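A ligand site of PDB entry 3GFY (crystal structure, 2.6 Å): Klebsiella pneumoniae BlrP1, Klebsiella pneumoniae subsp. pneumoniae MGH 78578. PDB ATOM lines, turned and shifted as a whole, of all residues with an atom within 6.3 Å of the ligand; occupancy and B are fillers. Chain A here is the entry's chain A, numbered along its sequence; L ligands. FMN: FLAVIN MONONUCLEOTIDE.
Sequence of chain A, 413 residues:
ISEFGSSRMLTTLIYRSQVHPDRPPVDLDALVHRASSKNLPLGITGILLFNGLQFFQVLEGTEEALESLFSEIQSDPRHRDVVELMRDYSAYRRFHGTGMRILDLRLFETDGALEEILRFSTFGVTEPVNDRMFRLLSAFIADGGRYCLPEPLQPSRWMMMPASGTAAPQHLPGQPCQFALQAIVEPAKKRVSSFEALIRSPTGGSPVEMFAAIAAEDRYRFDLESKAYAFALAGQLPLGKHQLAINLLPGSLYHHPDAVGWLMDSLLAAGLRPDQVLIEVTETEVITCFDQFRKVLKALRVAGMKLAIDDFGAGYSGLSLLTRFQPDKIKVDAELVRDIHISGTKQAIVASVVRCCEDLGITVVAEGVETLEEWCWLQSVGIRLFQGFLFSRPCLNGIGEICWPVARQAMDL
O2' of the ligand lies within hydrogen-bond range of OD2 of Asp 76 (2.7 Å).
The side-chain amide oxygen of Asn 39 lies within hydrogen-bond range of a nitrogen (N3) of the ligand, at 2.8 Å.
The guanidinium group (NE) of Arg 34 lies within salt-bridge range of an oxygen (O3P) of the ligand.
An oxygen (O2P) of the ligand lies within salt-bridge range of the side-chain amino group of Lys 38, at 3.8 Å.
NE2 of Gln 57 is in hydrogen-bond range of N5 of the ligand.
The guanidinium group (NH1) of Arg 78 is in hydrogen-bond range of an oxygen (O3') of the ligand, 3.4 Å away.
An oxygen (O2') of the ligand sits at hydrogen-bond distance from the backbone carbonyl oxygen of Glu 72 (3.4 Å).
The side-chain amide oxygen of Asn 39 sits close to the backbone carbonyl oxygen of Ala 35 (3.4 Å).
The side-chain amide nitrogen (ND2) of Asn 39 sits at hydrogen-bond distance from the backbone carbonyl oxygen (O) of Gly 99.
The backbone carbonyl oxygen (O) of Asn 39 lies within hydrogen-bond range of the backbone NH (N) of Ile 44, at 2.8 Å.
OE1 of Gln 57 sits at hydrogen-bond distance from OH of Tyr 15 (2.6 Å).
NE2 of Gln 57 sits close to SD of Met 100 (3.4 Å).
NE2 of His 79 lies within hydrogen-bond range of O of Ile 73 (2.8 Å).
A ring nitrogen (ND1) of His 79 sits at hydrogen-bond distance from the side-chain hydroxyl (OG) of Ser 17 (2.7 Å).
The backbone carbonyl oxygen (O) of Ser 17 sits at hydrogen-bond distance from the backbone NH (N) of Phe 55 (2.9 Å).
Merely in contact with the ligand: Tyr 15, Ala 35, Ile 73, Leu 69, Met 100, His 79, Leu 59, Leu 31, Phe 55 and Leu 48.
Hydrophobic or aromatic side chains that line the ligand: Leu 31, Ala 35, Leu 48, Phe 55, Leu 59, Leu 69, Ile 73, His 79 and Met 100.
17 residues have an atom within 4 Å of the ligand: Tyr 15, Leu 31, Arg 34, Ala 35, Lys 38, Asn 39, Leu 48, Phe 55, Gln 57, Leu 59, Leu 69, Glu 72, Ile 73, Asp 76, Arg 78, His 79 and Met 100.
Along chain A the residues within 4 Å of the ligand span positions 15 to 100.
The nearest printed residue that does not touch the ligand is Ser 17 (4.7 Å).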
ATOM      1  N   TYR A  15     -29.832 -36.961 -13.099  1.00  0.00           N
ATOM      2  CA  TYR A  15     -28.506 -37.101 -13.687  1.00  0.00           C
ATOM      3  C   TYR A  15     -27.420 -36.526 -12.799  1.00  0.00           C
ATOM      4  O   TYR A  15     -27.678 -35.653 -11.966  1.00  0.00           O
ATOM      5  CB  TYR A  15     -28.441 -36.458 -15.087  1.00  0.00           C
ATOM      6  CG  TYR A  15     -28.409 -34.946 -15.093  1.00  0.00           C
ATOM      7  CD1 TYR A  15     -27.205 -34.255 -14.925  1.00  0.00           C
ATOM      8  CD2 TYR A  15     -29.564 -34.206 -15.290  1.00  0.00           C
ATOM      9  CE1 TYR A  15     -27.167 -32.869 -14.932  1.00  0.00           C
ATOM     10  CE2 TYR A  15     -29.533 -32.817 -15.318  1.00  0.00           C
ATOM     11  CZ  TYR A  15     -28.325 -32.157 -15.123  1.00  0.00           C
ATOM     12  OH  TYR A  15     -28.280 -30.786 -15.131  1.00  0.00           O
ATOM     13  N   SER A  17     -23.447 -34.753 -13.255  1.00  0.00           N
ATOM     14  CA  SER A  17     -22.471 -34.209 -14.200  1.00  0.00           C
ATOM     15  C   SER A  17     -21.262 -33.635 -13.468  1.00  0.00           C
ATOM     16  O   SER A  17     -21.189 -33.675 -12.234  1.00  0.00           O
ATOM     17  CB  SER A  17     -23.119 -33.151 -15.103  1.00  0.00           C
ATOM     18  OG  SER A  17     -23.418 -31.962 -14.402  1.00  0.00           O
ATOM     19  N   VAL A  26     -18.710 -21.122 -12.737  1.00  0.00           N
ATOM     20  CA  VAL A  26     -20.023 -20.755 -13.238  1.00  0.00           C
ATOM     21  C   VAL A  26     -20.813 -20.030 -12.147  1.00  0.00           C
ATOM     22  O   VAL A  26     -20.813 -20.457 -11.000  1.00  0.00           O
ATOM     23  CB  VAL A  26     -20.797 -22.008 -13.707  1.00  0.00           C
ATOM     24  CG1 VAL A  26     -22.053 -21.602 -14.470  1.00  0.00           C
ATOM     25  CG2 VAL A  26     -19.918 -22.887 -14.579  1.00  0.00           C
ATOM     26  N   LEU A  28     -23.637 -19.789 -10.343  1.00  0.00           N
ATOM     27  CA  LEU A  28     -24.716 -20.741 -10.090  1.00  0.00           C
ATOM     28  C   LEU A  28     -25.987 -20.066  -9.593  1.00  0.00           C
ATOM     29  O   LEU A  28     -27.081 -20.606  -9.785  1.00  0.00           O
ATOM     30  CB  LEU A  28     -24.251 -21.825  -9.108  1.00  0.00           C
ATOM     31  CG  LEU A  28     -23.105 -22.709  -9.618  1.00  0.00           C
ATOM     32  CD1 LEU A  28     -22.581 -23.593  -8.513  1.00  0.00           C
ATOM     33  CD2 LEU A  28     -23.537 -23.544 -10.818  1.00  0.00           C
ATOM     34  N   LEU A  31     -27.770 -19.027 -12.803  1.00  0.00           N
ATOM     35  CA  LEU A  31     -28.284 -20.233 -13.468  1.00  0.00           C
ATOM     36  C   LEU A  31     -29.557 -20.750 -12.813  1.00  0.00           C
ATOM     37  O   LEU A  31     -30.566 -20.931 -13.499  1.00  0.00           O
ATOM     38  CB  LEU A  31     -27.210 -21.322 -13.504  1.00  0.00           C
ATOM     39  CG  LEU A  31     -27.474 -22.623 -14.263  1.00  0.00           C
ATOM     40  CD1 LEU A  31     -26.190 -23.123 -14.903  1.00  0.00           C
ATOM     41  CD2 LEU A  31     -28.075 -23.716 -13.384  1.00  0.00           C
ATOM     42  N   ARG A  34     -32.545 -18.359 -12.998  1.00  0.00           N
ATOM     43  CA  ARG A  34     -33.037 -18.423 -14.371  1.00  0.00           C
ATOM     44  C   ARG A  34     -33.745 -19.752 -14.610  1.00  0.00           C
ATOM     45  O   ARG A  34     -34.798 -19.801 -15.256  1.00  0.00           O
ATOM     46  CB  ARG A  34     -31.890 -18.257 -15.372  1.00  0.00           C
ATOM     47  CG  ARG A  34     -32.341 -17.897 -16.784  1.00  0.00           C
ATOM     48  CD  ARG A  34     -31.156 -17.752 -17.736  1.00  0.00           C
ATOM     49  NE  ARG A  34     -31.565 -17.143 -19.011  1.00  0.00           N
ATOM     50  CZ  ARG A  34     -31.389 -15.863 -19.327  1.00  0.00           C
ATOM     51  NH1 ARG A  34     -30.792 -15.037 -18.474  1.00  0.00           N
ATOM     52  NH2 ARG A  34     -31.801 -15.411 -20.499  1.00  0.00           N
ATOM     53  N   ALA A  35     -33.176 -20.834 -14.076  1.00  0.00           N
ATOM     54  CA  ALA A  35     -33.748 -22.169 -14.194  1.00  0.00           C
ATOM     55  C   ALA A  35     -35.110 -22.247 -13.524  1.00  0.00           C
ATOM     56  O   ALA A  35     -36.060 -22.742 -14.119  1.00  0.00           O
ATOM     57  CB  ALA A  35     -32.804 -23.217 -13.622  1.00  0.00           C
ATOM     58  N   SER A  36     -35.186 -21.749 -12.289  1.00  0.00           N
ATOM     59  CA  SER A  36     -36.416 -21.791 -11.503  1.00  0.00           C
ATOM     60  C   SER A  36     -37.546 -21.011 -12.176  1.00  0.00           C
ATOM     61  O   SER A  36     -38.693 -21.452 -12.198  1.00  0.00           O
ATOM     62  CB  SER A  36     -36.158 -21.231 -10.100  1.00  0.00           C
ATOM     63  OG  SER A  36     -37.121 -21.717  -9.181  1.00  0.00           O
ATOM     64  N   LYS A  38     -37.797 -20.351 -15.397  1.00  0.00           N
ATOM     65  CA  LYS A  38     -38.177 -20.993 -16.651  1.00  0.00           C
ATOM     66  C   LYS A  38     -38.929 -22.307 -16.410  1.00  0.00           C
ATOM     67  O   LYS A  38     -39.870 -22.622 -17.131  1.00  0.00           O
ATOM     68  CB  LYS A  38     -36.936 -21.220 -17.514  1.00  0.00           C
ATOM     69  CG  LYS A  38     -37.204 -21.489 -18.986  1.00  0.00           C
ATOM     70  CD  LYS A  38     -35.900 -21.752 -19.729  1.00  0.00           C
ATOM     71  CE  LYS A  38     -36.154 -22.305 -21.127  1.00  0.00           C
ATOM     72  NZ  LYS A  38     -34.993 -23.111 -21.612  1.00  0.00           N
ATOM     73  N   ASN A  39     -38.504 -23.039 -15.384  1.00  0.00           N
ATOM     74  CA  ASN A  39     -39.056 -24.372 -15.071  1.00  0.00           C
ATOM     75  C   ASN A  39     -40.501 -24.390 -14.611  1.00  0.00           C
ATOM     76  O   ASN A  39     -41.302 -25.174 -15.122  1.00  0.00           O
ATOM     77  CB  ASN A  39     -38.193 -25.071 -14.012  1.00  0.00           C
ATOM     78  CG  ASN A  39     -36.922 -25.669 -14.580  1.00  0.00           C
ATOM     79  OD1 ASN A  39     -36.670 -25.606 -15.783  1.00  0.00           O
ATOM     80  ND2 ASN A  39     -36.094 -26.233 -13.705  1.00  0.00           N
ATOM     81  N   ILE A  44     -42.202 -27.804 -14.609  1.00  0.00           N
ATOM     82  CA  ILE A  44     -40.977 -28.519 -14.251  1.00  0.00           C
ATOM     83  C   ILE A  44     -40.534 -28.113 -12.853  1.00  0.00           C
ATOM     84  O   ILE A  44     -40.481 -26.925 -12.530  1.00  0.00           O
ATOM     85  CB  ILE A  44     -39.838 -28.254 -15.269  1.00  0.00           C
ATOM     86  CG1 ILE A  44     -40.264 -28.678 -16.671  1.00  0.00           C
ATOM     87  CG2 ILE A  44     -38.552 -28.960 -14.846  1.00  0.00           C
ATOM     88  CD1 ILE A  44     -39.348 -28.179 -17.793  1.00  0.00           C
ATOM     89  N   LEU A  48     -31.017 -29.075  -7.471  1.00  0.00           N
ATOM     90  CA  LEU A  48     -29.649 -29.243  -7.915  1.00  0.00           C
ATOM     91  C   LEU A  48     -28.746 -29.366  -6.704  1.00  0.00           C
ATOM     92  O   LEU A  48     -28.812 -28.550  -5.774  1.00  0.00           O
ATOM     93  CB  LEU A  48     -29.230 -28.065  -8.799  1.00  0.00           C
ATOM     94  CG  LEU A  48     -27.819 -28.054  -9.392  1.00  0.00           C
ATOM     95  CD1 LEU A  48     -27.628 -29.181 -10.395  1.00  0.00           C
ATOM     96  CD2 LEU A  48     -27.522 -26.710 -10.042  1.00  0.00           C
ATOM     97  N   PHE A  55     -22.332 -31.855 -10.281  1.00  0.00           N
ATOM     98  CA  PHE A  55     -23.744 -31.529 -10.163  1.00  0.00           C
ATOM     99  C   PHE A  55     -24.583 -32.806 -10.048  1.00  0.00           C
ATOM    100  O   PHE A  55     -24.193 -33.858 -10.541  1.00  0.00           O
ATOM    101  CB  PHE A  55     -24.244 -30.741 -11.378  1.00  0.00           C
ATOM    102  CG  PHE A  55     -23.568 -29.426 -11.563  1.00  0.00           C
ATOM    103  CD1 PHE A  55     -23.822 -28.372 -10.705  1.00  0.00           C
ATOM    104  CD2 PHE A  55     -22.682 -29.231 -12.626  1.00  0.00           C
ATOM    105  CE1 PHE A  55     -23.194 -27.152 -10.880  1.00  0.00           C
ATOM    106  CE2 PHE A  55     -22.058 -28.019 -12.806  1.00  0.00           C
ATOM    107  CZ  PHE A  55     -22.308 -26.976 -11.932  1.00  0.00           C
ATOM    108  N   GLN A  57     -28.817 -33.406 -10.415  1.00  0.00           N
ATOM    109  CA  GLN A  57     -30.080 -32.731 -10.629  1.00  0.00           C
ATOM    110  C   GLN A  57     -31.249 -33.683 -10.738  1.00  0.00           C
ATOM    111  O   GLN A  57     -31.175 -34.699 -11.435  1.00  0.00           O
ATOM    112  CB  GLN A  57     -30.012 -31.814 -11.864  1.00  0.00           C
ATOM    113  CG  GLN A  57     -31.196 -30.878 -11.992  1.00  0.00           C
ATOM    114  CD  GLN A  57     -30.962 -29.769 -13.001  1.00  0.00           C
ATOM    115  OE1 GLN A  57     -30.588 -30.014 -14.150  1.00  0.00           O
ATOM    116  NE2 GLN A  57     -31.200 -28.532 -12.580  1.00  0.00           N
ATOM    117  N   LEU A  59     -35.128 -33.669 -11.990  1.00  0.00           N
ATOM    118  CA  LEU A  59     -36.136 -32.931 -12.748  1.00  0.00           C
ATOM    119  C   LEU A  59     -37.453 -33.693 -12.750  1.00  0.00           C
ATOM    120  O   LEU A  59     -37.483 -34.898 -12.954  1.00  0.00           O
ATOM    121  CB  LEU A  59     -35.673 -32.696 -14.198  1.00  0.00           C
ATOM    122  CG  LEU A  59     -34.520 -31.708 -14.420  1.00  0.00           C
ATOM    123  CD1 LEU A  59     -33.941 -31.868 -15.812  1.00  0.00           C
ATOM    124  CD2 LEU A  59     -34.977 -30.265 -14.186  1.00  0.00           C
ATOM    125  N   LEU A  69     -35.938 -30.157 -22.293  1.00  0.00           N
ATOM    126  CA  LEU A  69     -35.047 -29.459 -21.381  1.00  0.00           C
ATOM    127  C   LEU A  69     -33.698 -30.175 -21.205  1.00  0.00           C
ATOM    128  O   LEU A  69     -32.646 -29.545 -21.326  1.00  0.00           O
ATOM    129  CB  LEU A  69     -35.722 -29.243 -20.012  1.00  0.00           C
ATOM    130  CG  LEU A  69     -34.844 -28.735 -18.868  1.00  0.00           C
ATOM    131  CD1 LEU A  69     -34.294 -27.352 -19.159  1.00  0.00           C
ATOM    132  CD2 LEU A  69     -35.607 -28.766 -17.561  1.00  0.00           C
ATOM    133  N   GLU A  72     -31.302 -29.528 -23.937  1.00  0.00           N
ATOM    134  CA  GLU A  72     -30.583 -28.258 -23.777  1.00  0.00           C
ATOM    135  C   GLU A  72     -29.471 -28.379 -22.731  1.00  0.00           C
ATOM    136  O   GLU A  72     -28.409 -27.783 -22.890  1.00  0.00           O
ATOM    137  CB  GLU A  72     -31.547 -27.129 -23.381  1.00  0.00           C
ATOM    138  CG  GLU A  72     -32.216 -26.391 -24.550  1.00  0.00           C
ATOM    139  CD  GLU A  72     -33.212 -25.317 -24.097  1.00  0.00           C
ATOM    140  OE1 GLU A  72     -34.116 -25.631 -23.285  1.00  0.00           O
ATOM    141  OE2 GLU A  72     -33.095 -24.154 -24.552  1.00  0.00           O
ATOM    142  N   ILE A  73     -29.747 -29.150 -21.676  1.00  0.00           N
ATOM    143  CA  ILE A  73     -28.798 -29.365 -20.578  1.00  0.00           C
ATOM    144  C   ILE A  73     -27.586 -30.206 -21.001  1.00  0.00           C
ATOM    145  O   ILE A  73     -26.453 -29.926 -20.602  1.00  0.00           O
ATOM    146  CB  ILE A  73     -29.511 -29.993 -19.349  1.00  0.00           C
ATOM    147  CG1 ILE A  73     -30.275 -28.915 -18.568  1.00  0.00           C
ATOM    148  CG2 ILE A  73     -28.520 -30.704 -18.431  1.00  0.00           C
ATOM    149  CD1 ILE A  73     -31.262 -29.447 -17.550  1.00  0.00           C
ATOM    150  N   GLN A  74     -27.828 -31.232 -21.823  1.00  0.00           N
ATOM    151  CA  GLN A  74     -26.762 -32.085 -22.327  1.00  0.00           C
ATOM    152  C   GLN A  74     -25.747 -31.343 -23.195  1.00  0.00           C
ATOM    153  O   GLN A  74     -24.555 -31.644 -23.164  1.00  0.00           O
ATOM    154  CB  GLN A  74     -27.341 -33.269 -23.110  1.00  0.00           C
ATOM    155  CG  GLN A  74     -27.805 -34.417 -22.243  1.00  0.00           C
ATOM    156  CD  GLN A  74     -28.288 -35.579 -23.072  1.00  0.00           C
ATOM    157  OE1 GLN A  74     -29.252 -35.468 -23.828  1.00  0.00           O
ATOM    158  NE2 GLN A  74     -27.626 -36.724 -22.929  1.00  0.00           N
ATOM    159  N   SER A  75     -26.233 -30.364 -23.958  1.00  0.00           N
ATOM    160  CA  SER A  75     -25.385 -29.581 -24.853  1.00  0.00           C
ATOM    161  C   SER A  75     -24.853 -28.295 -24.212  1.00  0.00           C
ATOM    162  O   SER A  75     -24.256 -27.452 -24.889  1.00  0.00           O
ATOM    163  CB  SER A  75     -26.120 -29.271 -26.152  1.00  0.00           C
ATOM    164  OG  SER A  75     -26.382 -30.450 -26.889  1.00  0.00           O
ATOM    165  N   ASP A  76     -25.079 -28.135 -22.899  1.00  0.00           N
ATOM    166  CA  ASP A  76     -24.605 -26.969 -22.177  1.00  0.00           C
ATOM    167  C   ASP A  76     -23.098 -27.090 -21.866  1.00  0.00           C
ATOM    168  O   ASP A  76     -22.686 -28.045 -21.216  1.00  0.00           O
ATOM    169  CB  ASP A  76     -25.408 -26.787 -20.886  1.00  0.00           C
ATOM    170  CG  ASP A  76     -25.286 -25.391 -20.311  1.00  0.00           C
ATOM    171  OD1 ASP A  76     -24.156 -24.889 -20.144  1.00  0.00           O
ATOM    172  OD2 ASP A  76     -26.337 -24.784 -19.993  1.00  0.00           O
ATOM    173  N   ARG A  78     -21.275 -25.390 -19.829  1.00  0.00           N
ATOM    174  CA  ARG A  78     -20.915 -25.056 -18.435  1.00  0.00           C
ATOM    175  C   ARG A  78     -20.591 -26.295 -17.610  1.00  0.00           C
ATOM    176  O   ARG A  78     -19.959 -26.207 -16.556  1.00  0.00           O
ATOM    177  CB  ARG A  78     -22.058 -24.321 -17.731  1.00  0.00           C
ATOM    178  CG  ARG A  78     -22.470 -22.976 -18.285  1.00  0.00           C
ATOM    179  CD  ARG A  78     -23.736 -22.591 -17.567  1.00  0.00           C
ATOM    180  NE  ARG A  78     -24.372 -21.370 -18.012  1.00  0.00           N
ATOM    181  CZ  ARG A  78     -25.639 -21.291 -18.414  1.00  0.00           C
ATOM    182  NH1 ARG A  78     -26.392 -22.382 -18.453  1.00  0.00           N
ATOM    183  NH2 ARG A  78     -26.142 -20.128 -18.797  1.00  0.00           N
ATOM    184  N   HIS A  79     -21.047 -27.457 -18.074  1.00  0.00           N
ATOM    185  CA  HIS A  79     -20.694 -28.711 -17.441  1.00  0.00           C
ATOM    186  C   HIS A  79     -20.377 -29.782 -18.488  1.00  0.00           C
ATOM    187  O   HIS A  79     -20.559 -29.558 -19.679  1.00  0.00           O
ATOM    188  CB  HIS A  79     -21.767 -29.162 -16.432  1.00  0.00           C
ATOM    189  CG  HIS A  79     -23.087 -29.541 -17.051  1.00  0.00           C
ATOM    190  ND1 HIS A  79     -24.093 -30.134 -16.319  1.00  0.00           N
ATOM    191  CD2 HIS A  79     -23.560 -29.419 -18.311  1.00  0.00           C
ATOM    192  CE1 HIS A  79     -25.128 -30.359 -17.103  1.00  0.00           C
ATOM    193  NE2 HIS A  79     -24.837 -29.937 -18.315  1.00  0.00           N
ATOM    194  N   GLY A  99     -39.306 -24.502  -8.694  1.00  0.00           N
ATOM    195  CA  GLY A  99     -38.857 -24.539 -10.091  1.00  0.00           C
ATOM    196  C   GLY A  99     -37.487 -25.168 -10.208  1.00  0.00           C
ATOM    197  O   GLY A  99     -37.296 -26.146 -10.935  1.00  0.00           O
ATOM    198  N   MET A 100     -36.539 -24.594  -9.471  1.00  0.00           N
ATOM    199  CA  MET A 100     -35.201 -25.153  -9.320  1.00  0.00           C
ATOM    200  C   MET A 100     -34.560 -24.525  -8.094  1.00  0.00           C
ATOM    201  O   MET A 100     -34.818 -23.359  -7.792  1.00  0.00           O
ATOM    202  CB  MET A 100     -34.346 -24.912 -10.568  1.00  0.00           C
ATOM    203  CG  MET A 100     -33.033 -25.699 -10.606  1.00  0.00           C
ATOM    204  SD  MET A 100     -33.142 -27.419 -10.028  1.00  0.00           S
ATOM    205  CE  MET A 100     -34.280 -28.148 -11.209  1.00  0.00           C
HETATM  206  N1  FMN L   1     -32.138 -24.615 -17.546  1.00  0.00           N
HETATM  207  C2  FMN L   1     -33.475 -24.642 -17.195  1.00  0.00           C
HETATM  208  O2  FMN L   1     -34.275 -23.991 -17.856  1.00  0.00           O
HETATM  209  N3  FMN L   1     -33.908 -25.400 -16.129  1.00  0.00           N
HETATM  210  C4  FMN L   1     -32.999 -26.141 -15.397  1.00  0.00           C
HETATM  211  O4  FMN L   1     -33.404 -26.907 -14.529  1.00  0.00           O
HETATM  212  C4A FMN L   1     -31.649 -26.107 -15.746  1.00  0.00           C
HETATM  213  N5  FMN L   1     -30.726 -26.828 -15.017  1.00  0.00           N
HETATM  214  C5A FMN L   1     -29.394 -26.810 -15.348  1.00  0.00           C
HETATM  215  C6  FMN L   1     -28.490 -27.560 -14.596  1.00  0.00           C
HETATM  216  C7  FMN L   1     -27.132 -27.549 -14.914  1.00  0.00           C
HETATM  217  C7M FMN L   1     -26.170 -28.147 -13.935  1.00  0.00           C
HETATM  218  C8  FMN L   1     -26.687 -26.798 -16.000  1.00  0.00           C
HETATM  219  C8M FMN L   1     -25.204 -26.618 -16.234  1.00  0.00           C
HETATM  220  C9  FMN L   1     -27.594 -26.056 -16.757  1.00  0.00           C
HETATM  221  C9A FMN L   1     -28.951 -26.053 -16.443  1.00  0.00           C
HETATM  222  N10 FMN L   1     -29.873 -25.318 -17.176  1.00  0.00           N
HETATM  223  C10 FMN L   1     -31.219 -25.344 -16.821  1.00  0.00           C
HETATM  224  C1' FMN L   1     -29.411 -24.417 -18.300  1.00  0.00           C
HETATM  225  C2' FMN L   1     -29.722 -25.036 -19.668  1.00  0.00           C
HETATM  226  O2' FMN L   1     -28.729 -25.972 -20.012  1.00  0.00           O
HETATM  227  C3' FMN L   1     -29.807 -23.984 -20.782  1.00  0.00           C
HETATM  228  O3' FMN L   1     -28.604 -23.257 -20.825  1.00  0.00           O
HETATM  229  C4' FMN L   1     -30.985 -23.025 -20.610  1.00  0.00           C
HETATM  230  O4' FMN L   1     -32.148 -23.726 -20.236  1.00  0.00           O
HETATM  231  C5' FMN L   1     -31.239 -22.263 -21.907  1.00  0.00           C
HETATM  232  O5' FMN L   1     -32.454 -21.559 -21.802  1.00  0.00           O
HETATM  233  P   FMN L   1     -32.496 -19.954 -21.849  1.00  0.00           P
HETATM  234  O1P FMN L   1     -31.864 -19.505 -23.156  1.00  0.00           O
HETATM  235  O2P FMN L   1     -33.936 -19.480 -21.771  1.00  0.00           O
HETATM  236  O3P FMN L   1     -31.719 -19.387 -20.687  1.00  0.00           O
